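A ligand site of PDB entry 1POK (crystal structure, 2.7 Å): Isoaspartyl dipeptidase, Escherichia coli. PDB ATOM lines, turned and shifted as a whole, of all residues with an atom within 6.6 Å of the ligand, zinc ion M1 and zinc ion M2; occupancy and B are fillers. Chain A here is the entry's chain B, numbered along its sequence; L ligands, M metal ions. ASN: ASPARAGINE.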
ATOM      1  N   HIS A  68      30.147  -6.126 -19.659  1.00  0.00           N
ATOM      2  CA  HIS A  68      29.369  -6.159 -20.897  1.00  0.00           C
ATOM      3  C   HIS A  68      29.962  -7.192 -21.835  1.00  0.00           C
ATOM      4  O   HIS A  68      30.720  -6.856 -22.743  1.00  0.00           O
ATOM      5  CB  HIS A  68      29.400  -4.786 -21.571  1.00  0.00           C
ATOM      6  CG  HIS A  68      28.196  -4.489 -22.393  1.00  0.00           C
ATOM      7  ND1 HIS A  68      27.078  -3.876 -21.876  1.00  0.00           N
ATOM      8  CD2 HIS A  68      27.921  -4.711 -23.702  1.00  0.00           C
ATOM      9  CE1 HIS A  68      26.163  -3.732 -22.826  1.00  0.00           C
ATOM     10  NE2 HIS A  68      26.653  -4.228 -23.938  1.00  0.00           N
ATOM     11  N   HIS A  70      29.056 -10.774 -24.184  1.00  0.00           N
ATOM     12  CA  HIS A  70      28.140 -11.773 -24.692  1.00  0.00           C
ATOM     13  C   HIS A  70      28.864 -13.094 -24.516  1.00  0.00           C
ATOM     14  O   HIS A  70      29.402 -13.637 -25.475  1.00  0.00           O
ATOM     15  CB  HIS A  70      27.840 -11.478 -26.164  1.00  0.00           C
ATOM     16  CG  HIS A  70      27.269 -10.112 -26.385  1.00  0.00           C
ATOM     17  ND1 HIS A  70      25.938  -9.828 -26.165  1.00  0.00           N
ATOM     18  CD2 HIS A  70      27.873  -8.921 -26.636  1.00  0.00           C
ATOM     19  CE1 HIS A  70      25.749  -8.521 -26.270  1.00  0.00           C
ATOM     20  NE2 HIS A  70      26.904  -7.947 -26.549  1.00  0.00           N
ATOM     21  N   GLU A  77      22.676 -10.472 -36.372  1.00  0.00           N
ATOM     22  CA  GLU A  77      21.949  -9.350 -36.959  1.00  0.00           C
ATOM     23  C   GLU A  77      21.999  -9.312 -38.491  1.00  0.00           C
ATOM     24  O   GLU A  77      21.530  -8.366 -39.123  1.00  0.00           O
ATOM     25  CB  GLU A  77      22.489  -8.058 -36.340  1.00  0.00           C
ATOM     26  CG  GLU A  77      22.529  -8.206 -34.807  1.00  0.00           C
ATOM     27  CD  GLU A  77      23.042  -6.982 -34.057  1.00  0.00           C
ATOM     28  OE1 GLU A  77      22.628  -5.850 -34.419  1.00  0.00           O
ATOM     29  OE2 GLU A  77      23.843  -7.157 -33.115  1.00  0.00           O
ATOM     30  N   LEU A 103      25.733 -11.143 -20.786  1.00  0.00           N
ATOM     31  CA  LEU A 103      24.440 -10.625 -21.176  1.00  0.00           C
ATOM     32  C   LEU A 103      24.130 -11.029 -22.613  1.00  0.00           C
ATOM     33  O   LEU A 103      24.998 -11.549 -23.323  1.00  0.00           O
ATOM     34  CB  LEU A 103      24.406  -9.092 -21.007  1.00  0.00           C
ATOM     35  CG  LEU A 103      25.166  -8.104 -21.917  1.00  0.00           C
ATOM     36  CD1 LEU A 103      25.452  -6.835 -21.119  1.00  0.00           C
ATOM     37  CD2 LEU A 103      26.473  -8.684 -22.405  1.00  0.00           C
ATOM     38  N   LEU A 104      22.881 -10.823 -23.015  1.00  0.00           N
ATOM     39  CA  LEU A 104      22.451 -11.150 -24.369  1.00  0.00           C
ATOM     40  C   LEU A 104      22.170  -9.851 -25.095  1.00  0.00           C
ATOM     41  O   LEU A 104      21.813  -8.859 -24.487  1.00  0.00           O
ATOM     42  CB  LEU A 104      21.193 -12.017 -24.331  1.00  0.00           C
ATOM     43  CG  LEU A 104      21.307 -13.417 -23.725  1.00  0.00           C
ATOM     44  CD1 LEU A 104      19.921 -14.030 -23.652  1.00  0.00           C
ATOM     45  CD2 LEU A 104      22.240 -14.279 -24.542  1.00  0.00           C
ATOM     46  N   GLY A 105      22.313  -9.874 -26.420  1.00  0.00           N
ATOM     47  CA  GLY A 105      22.097  -8.671 -27.203  1.00  0.00           C
ATOM     48  C   GLY A 105      20.811  -8.692 -27.991  1.00  0.00           C
ATOM     49  O   GLY A 105      19.747  -8.981 -27.451  1.00  0.00           O
ATOM     50  N   THR A 106      20.913  -8.391 -29.283  1.00  0.00           N
ATOM     51  CA  THR A 106      19.748  -8.351 -30.167  1.00  0.00           C
ATOM     52  C   THR A 106      19.049  -9.688 -30.307  1.00  0.00           C
ATOM     53  O   THR A 106      17.835  -9.783 -30.166  1.00  0.00           O
ATOM     54  CB  THR A 106      20.137  -7.899 -31.564  1.00  0.00           C
ATOM     55  OG1 THR A 106      21.149  -6.889 -31.479  1.00  0.00           O
ATOM     56  CG2 THR A 106      18.920  -7.361 -32.281  1.00  0.00           C
ATOM     57  N   TYR A 137      17.746  -7.067 -25.603  1.00  0.00           N
ATOM     58  CA  TYR A 137      17.210  -5.825 -26.183  1.00  0.00           C
ATOM     59  C   TYR A 137      15.694  -5.797 -26.023  1.00  0.00           C
ATOM     60  O   TYR A 137      15.108  -4.727 -25.871  1.00  0.00           O
ATOM     61  CB  TYR A 137      17.492  -5.715 -27.694  1.00  0.00           C
ATOM     62  CG  TYR A 137      18.885  -5.266 -28.128  1.00  0.00           C
ATOM     63  CD1 TYR A 137      19.110  -4.908 -29.457  1.00  0.00           C
ATOM     64  CD2 TYR A 137      19.970  -5.246 -27.245  1.00  0.00           C
ATOM     65  CE1 TYR A 137      20.374  -4.530 -29.898  1.00  0.00           C
ATOM     66  CE2 TYR A 137      21.240  -4.877 -27.676  1.00  0.00           C
ATOM     67  CZ  TYR A 137      21.437  -4.520 -29.011  1.00  0.00           C
ATOM     68  OH  TYR A 137      22.699  -4.164 -29.472  1.00  0.00           O
ATOM     69  N   KCX A 162      18.719  -6.275 -18.492  1.00  0.00           N
ATOM     70  CA  KCX A 162      19.235  -5.529 -19.628  1.00  0.00           C
ATOM     71  CB  KCX A 162      20.276  -6.374 -20.372  1.00  0.00           C
ATOM     72  CG  KCX A 162      21.140  -5.639 -21.411  1.00  0.00           C
ATOM     73  CD  KCX A 162      20.561  -5.697 -22.800  1.00  0.00           C
ATOM     74  CE  KCX A 162      21.417  -4.895 -23.767  1.00  0.00           C
ATOM     75  NZ  KCX A 162      22.541  -5.633 -24.336  1.00  0.00           N
ATOM     76  C   KCX A 162      18.054  -5.232 -20.562  1.00  0.00           C
ATOM     77  O   KCX A 162      16.981  -5.787 -20.397  1.00  0.00           O
ATOM     78  CX  KCX A 162      23.575  -5.071 -24.966  1.00  0.00           C
ATOM     79  OQ1 KCX A 162      23.631  -3.818 -25.094  1.00  0.00           O
ATOM     80  OQ2 KCX A 162      24.507  -5.761 -25.451  1.00  0.00           O
ATOM     81  N   ASP A 167      16.989   2.741 -30.191  1.00  0.00           N
ATOM     82  CA  ASP A 167      17.721   1.936 -31.157  1.00  0.00           C
ATOM     83  C   ASP A 167      16.738   1.399 -32.203  1.00  0.00           C
ATOM     84  O   ASP A 167      15.534   1.285 -31.934  1.00  0.00           O
ATOM     85  CB  ASP A 167      18.394   0.779 -30.411  1.00  0.00           C
ATOM     86  CG  ASP A 167      19.369   0.024 -31.265  1.00  0.00           C
ATOM     87  OD1 ASP A 167      20.468   0.551 -31.515  1.00  0.00           O
ATOM     88  OD2 ASP A 167      19.034  -1.108 -31.673  1.00  0.00           O
ATOM     89  N   HIS A 168      17.240   1.066 -33.386  1.00  0.00           N
ATOM     90  CA  HIS A 168      16.393   0.566 -34.464  1.00  0.00           C
ATOM     91  C   HIS A 168      16.278  -0.965 -34.403  1.00  0.00           C
ATOM     92  O   HIS A 168      15.778  -1.594 -35.337  1.00  0.00           O
ATOM     93  CB  HIS A 168      16.982   0.982 -35.807  1.00  0.00           C
ATOM     94  CG  HIS A 168      18.294   0.328 -36.112  1.00  0.00           C
ATOM     95  ND1 HIS A 168      18.393  -0.870 -36.785  1.00  0.00           N
ATOM     96  CD2 HIS A 168      19.558   0.670 -35.758  1.00  0.00           C
ATOM     97  CE1 HIS A 168      19.664  -1.230 -36.850  1.00  0.00           C
ATOM     98  NE2 HIS A 168      20.392  -0.320 -36.235  1.00  0.00           N
ATOM     99  N   ARG A 169      16.727  -1.556 -33.300  1.00  0.00           N
ATOM    100  CA  ARG A 169      16.671  -3.005 -33.119  1.00  0.00           C
ATOM    101  C   ARG A 169      16.011  -3.332 -31.784  1.00  0.00           C
ATOM    102  O   ARG A 169      16.203  -4.416 -31.235  1.00  0.00           O
ATOM    103  CB  ARG A 169      18.071  -3.621 -33.125  1.00  0.00           C
ATOM    104  CG  ARG A 169      18.918  -3.253 -34.322  1.00  0.00           C
ATOM    105  CD  ARG A 169      20.221  -4.030 -34.334  1.00  0.00           C
ATOM    106  NE  ARG A 169      21.087  -3.734 -33.189  1.00  0.00           N
ATOM    107  CZ  ARG A 169      21.885  -2.671 -33.089  1.00  0.00           C
ATOM    108  NH1 ARG A 169      21.934  -1.789 -34.076  1.00  0.00           N
ATOM    109  NH2 ARG A 169      22.638  -2.512 -32.014  1.00  0.00           N
ATOM    110  N   HIS A 201      20.916  -0.504 -23.545  1.00  0.00           N
ATOM    111  CA  HIS A 201      21.740  -0.457 -24.745  1.00  0.00           C
ATOM    112  C   HIS A 201      21.293   0.792 -25.466  1.00  0.00           C
ATOM    113  O   HIS A 201      20.104   0.947 -25.771  1.00  0.00           O
ATOM    114  CB  HIS A 201      21.476  -1.665 -25.647  1.00  0.00           C
ATOM    115  CG  HIS A 201      21.854  -1.428 -27.077  1.00  0.00           C
ATOM    116  ND1 HIS A 201      23.147  -1.544 -27.538  1.00  0.00           N
ATOM    117  CD2 HIS A 201      21.119  -1.034 -28.142  1.00  0.00           C
ATOM    118  CE1 HIS A 201      23.191  -1.242 -28.827  1.00  0.00           C
ATOM    119  NE2 HIS A 201      21.972  -0.914 -29.213  1.00  0.00           N
ATOM    120  N   MET A 202      22.223   1.699 -25.737  1.00  0.00           N
ATOM    121  CA  MET A 202      21.875   2.933 -26.414  1.00  0.00           C
ATOM    122  C   MET A 202      22.051   2.822 -27.919  1.00  0.00           C
ATOM    123  O   MET A 202      23.066   2.313 -28.403  1.00  0.00           O
ATOM    124  CB  MET A 202      22.690   4.098 -25.855  1.00  0.00           C
ATOM    125  CG  MET A 202      22.337   4.443 -24.423  1.00  0.00           C
ATOM    126  SD  MET A 202      20.550   4.512 -24.151  1.00  0.00           S
ATOM    127  CE  MET A 202      20.096   5.806 -25.255  1.00  0.00           C
ATOM    128  N   ASP A 204      21.234   4.829 -31.941  1.00  0.00           N
ATOM    129  CA  ASP A 204      21.545   6.116 -32.562  1.00  0.00           C
ATOM    130  C   ASP A 204      20.309   6.956 -32.839  1.00  0.00           C
ATOM    131  O   ASP A 204      20.261   7.677 -33.832  1.00  0.00           O
ATOM    132  CB  ASP A 204      22.310   5.912 -33.868  1.00  0.00           C
ATOM    133  CG  ASP A 204      23.768   5.620 -33.631  1.00  0.00           C
ATOM    134  OD1 ASP A 204      24.334   6.218 -32.702  1.00  0.00           O
ATOM    135  OD2 ASP A 204      24.348   4.805 -34.389  1.00  0.00           O
ATOM    136  N   THR A 229      24.680   2.383 -21.798  1.00  0.00           N
ATOM    137  CA  THR A 229      25.943   1.946 -22.366  1.00  0.00           C
ATOM    138  C   THR A 229      26.105   2.456 -23.788  1.00  0.00           C
ATOM    139  O   THR A 229      25.148   2.924 -24.392  1.00  0.00           O
ATOM    140  CB  THR A 229      26.053   0.425 -22.418  1.00  0.00           C
ATOM    141  OG1 THR A 229      25.558  -0.113 -21.196  1.00  0.00           O
ATOM    142  CG2 THR A 229      27.489  -0.004 -22.572  1.00  0.00           C
ATOM    143  N   HIS A 230      27.324   2.335 -24.308  1.00  0.00           N
ATOM    144  CA  HIS A 230      27.646   2.790 -25.661  1.00  0.00           C
ATOM    145  C   HIS A 230      27.341   4.273 -25.815  1.00  0.00           C
ATOM    146  O   HIS A 230      27.000   4.725 -26.903  1.00  0.00           O
ATOM    147  CB  HIS A 230      26.837   2.023 -26.692  1.00  0.00           C
ATOM    148  CG  HIS A 230      27.048   0.541 -26.645  1.00  0.00           C
ATOM    149  ND1 HIS A 230      26.608  -0.224 -25.593  1.00  0.00           N
ATOM    150  CD2 HIS A 230      27.657  -0.304 -27.504  1.00  0.00           C
ATOM    151  CE1 HIS A 230      26.942  -1.490 -25.803  1.00  0.00           C
ATOM    152  NE2 HIS A 230      27.580  -1.559 -26.967  1.00  0.00           N
ATOM    153  N   ARG A 233      28.759   6.316 -28.651  1.00  0.00           N
ATOM    154  CA  ARG A 233      28.448   5.848 -30.010  1.00  0.00           C
ATOM    155  C   ARG A 233      28.147   6.994 -30.973  1.00  0.00           C
ATOM    156  O   ARG A 233      28.320   6.841 -32.185  1.00  0.00           O
ATOM    157  CB  ARG A 233      27.262   4.858 -29.996  1.00  0.00           C
ATOM    158  CG  ARG A 233      25.899   5.506 -29.861  1.00  0.00           C
ATOM    159  CD  ARG A 233      24.775   4.470 -29.895  1.00  0.00           C
ATOM    160  NE  ARG A 233      24.776   3.682 -31.128  1.00  0.00           N
ATOM    161  CZ  ARG A 233      25.170   2.419 -31.209  1.00  0.00           C
ATOM    162  NH1 ARG A 233      25.592   1.754 -30.142  1.00  0.00           N
ATOM    163  NH2 ARG A 233      25.156   1.806 -32.389  1.00  0.00           N
ATOM    164  N   THR A 254      31.847   2.030 -24.032  1.00  0.00           N
ATOM    165  CA  THR A 254      32.341   0.772 -24.586  1.00  0.00           C
ATOM    166  C   THR A 254      33.664   0.942 -25.321  1.00  0.00           C
ATOM    167  O   THR A 254      33.790   1.739 -26.254  1.00  0.00           O
ATOM    168  CB  THR A 254      31.289   0.103 -25.539  1.00  0.00           C
ATOM    169  OG1 THR A 254      30.671   1.103 -26.353  1.00  0.00           O
ATOM    170  CG2 THR A 254      30.211  -0.642 -24.719  1.00  0.00           C
ATOM    171  N   SER A 256      34.943  -0.880 -27.280  1.00  0.00           N
ATOM    172  CA  SER A 256      34.923  -1.515 -28.598  1.00  0.00           C
ATOM    173  C   SER A 256      34.516  -0.542 -29.691  1.00  0.00           C
ATOM    174  O   SER A 256      34.424  -0.912 -30.866  1.00  0.00           O
ATOM    175  CB  SER A 256      33.993  -2.736 -28.573  1.00  0.00           C
ATOM    176  OG  SER A 256      32.781  -2.440 -27.894  1.00  0.00           O
ATOM    177  N   ILE A 257      34.265   0.701 -29.294  1.00  0.00           N
ATOM    178  CA  ILE A 257      33.878   1.761 -30.217  1.00  0.00           C
ATOM    179  C   ILE A 257      34.983   2.822 -30.233  1.00  0.00           C
ATOM    180  O   ILE A 257      35.364   3.331 -29.175  1.00  0.00           O
ATOM    181  CB  ILE A 257      32.564   2.438 -29.769  1.00  0.00           C
ATOM    182  CG1 ILE A 257      31.465   1.390 -29.615  1.00  0.00           C
ATOM    183  CG2 ILE A 257      32.150   3.480 -30.769  1.00  0.00           C
ATOM    184  CD1 ILE A 257      30.075   1.966 -29.277  1.00  0.00           C
ATOM    185  N   ASP A 285      31.959  -5.109 -24.443  1.00  0.00           N
ATOM    186  CA  ASP A 285      30.930  -5.583 -25.345  1.00  0.00           C
ATOM    187  C   ASP A 285      31.600  -6.658 -26.197  1.00  0.00           C
ATOM    188  O   ASP A 285      31.267  -6.838 -27.377  1.00  0.00           O
ATOM    189  CB  ASP A 285      30.389  -4.436 -26.199  1.00  0.00           C
ATOM    190  CG  ASP A 285      29.153  -4.838 -26.984  1.00  0.00           C
ATOM    191  OD1 ASP A 285      28.344  -5.630 -26.444  1.00  0.00           O
ATOM    192  OD2 ASP A 285      28.990  -4.362 -28.131  1.00  0.00           O
ATOM    193  N   GLY A 288      30.796  -9.433 -29.369  1.00  0.00           N
ATOM    194  CA  GLY A 288      29.594  -8.872 -29.954  1.00  0.00           C
ATOM    195  C   GLY A 288      29.740  -8.660 -31.446  1.00  0.00           C
ATOM    196  O   GLY A 288      29.968  -9.605 -32.202  1.00  0.00           O
ATOM    197  N   SER A 289      29.619  -7.394 -31.866  1.00  0.00           N
ATOM    198  CA  SER A 289      29.706  -6.972 -33.267  1.00  0.00           C
ATOM    199  C   SER A 289      28.386  -7.256 -33.972  1.00  0.00           C
ATOM    200  O   SER A 289      27.327  -6.773 -33.554  1.00  0.00           O
ATOM    201  CB  SER A 289      30.848  -7.695 -33.993  1.00  0.00           C
ATOM    202  OG  SER A 289      31.120  -7.110 -35.254  1.00  0.00           O
HETATM  203  N   ASN L   1      25.552  -1.638 -30.762  1.00  0.00           N
HETATM  204  CA  ASN L   1      25.611  -3.017 -31.332  1.00  0.00           C
HETATM  205  C   ASN L   1      26.495  -3.934 -30.483  1.00  0.00           C
HETATM  206  O   ASN L   1      26.519  -3.778 -29.244  1.00  0.00           O
HETATM  207  CB  ASN L   1      26.158  -2.961 -32.759  1.00  0.00           C
HETATM  208  CG  ASN L   1      25.520  -1.872 -33.593  1.00  0.00           C
HETATM  209  OD1 ASN L   1      25.830  -0.694 -33.448  1.00  0.00           O
HETATM  210  ND2 ASN L   1      24.624  -2.254 -34.482  1.00  0.00           N
HETATM  211  OXT ASN L   1      27.179  -4.794 -31.077  1.00  0.00           O
HETATM  212 ZN    ZN M   1      26.136  -5.454 -26.649  1.00  0.00          ZN
HETATM  213 ZN    ZN M   2      24.631  -3.273 -26.993  1.00  0.00          ZN
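OQ1 of KCX 162 binds zinc ion M2, at 2.2 Å. ND1 of His 201 binds zinc ion M2 (2.3 Å).
NE2 of His 68 sits close to OQ2 of KCX 162. The side-chain carboxylate (OD1) of Asp 285 sits close to a ring nitrogen (NE2) of His 70, at 2.7 Å. The backbone NH (N) of Asp 285 is in hydrogen-bond range of the backbone carbonyl oxygen (O) of His 68 (2.7 Å). The guanidinium group (NH2) of Arg 169 is in hydrogen-bond range of a ring nitrogen (NE2) of His 201 (3.3 Å). A ring nitrogen (NE2) of His 201 sits close to the side-chain hydroxyl of Tyr 137, at 3.3 Å. The guanidinium group of Arg 169 is in hydrogen-bond range of a ring nitrogen (NE2) of His 168 (3.0 Å). O of Met 202 is in hydrogen-bond range of NH1 of Arg 233, at 3.1 Å. The backbone carbonyl oxygen (O) of Gly 105 lies within hydrogen-bond range of the backbone NH (N) of Tyr 137.
The backbone carbonyl oxygen (O) of Ser 289 lies close to an oxygen (OXT) of the ligand (3.2 Å). Residues that only touch the ligand: Tyr 137 (3.6 Å). Hydrophobic or aromatic side chains within 4 Å of the ligand: His 201. Seven residues have an atom within 4 Å of the ligand: Tyr 137, Arg 169, His 201, His 230, Arg 233, Asp 285 and Ser 289.
His 68 touches zinc ion M2 (NE2 to ZN, 3.8 Å). OH of Tyr 137 touches zinc ion M2, 3.3 Å away. His 230 touches zinc ion M2. Within 4 Å of zinc ion M2: His 68, Tyr 137, KCX 162, His 201 and His 230. The nearest printed residue that does not touch zinc ion M2 is Asp 285 (4.4 Å).
His 68 touches zinc ion M1. Of the 24 residues printed, 4 come within 4 Å of zinc ion M1. The nearest printed residue that does not touch zinc ion M1 is His 230 (4.1 Å).
OD2 of Asp 285 lies close to O of the ligand. The guanidinium group (NH2) of Arg 169 sits close to a nitrogen (N) of the ligand. OD1 of the ligand is in hydrogen-bond range of NH2 of Arg 233 (2.8 Å). O of the ligand sits at hydrogen-bond distance from NE2 of His 230, at 3.4 Å.
Zinc ion M1 is bound by OQ2 of KCX 162 (2.0 Å) and the side-chain carboxylate of Asp 285 (2.2 Å). Zinc ion M1 has two donor atoms within binding distance. Slightly farther from zinc ion M1 lies NE2 of His 70 (2.6 Å).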
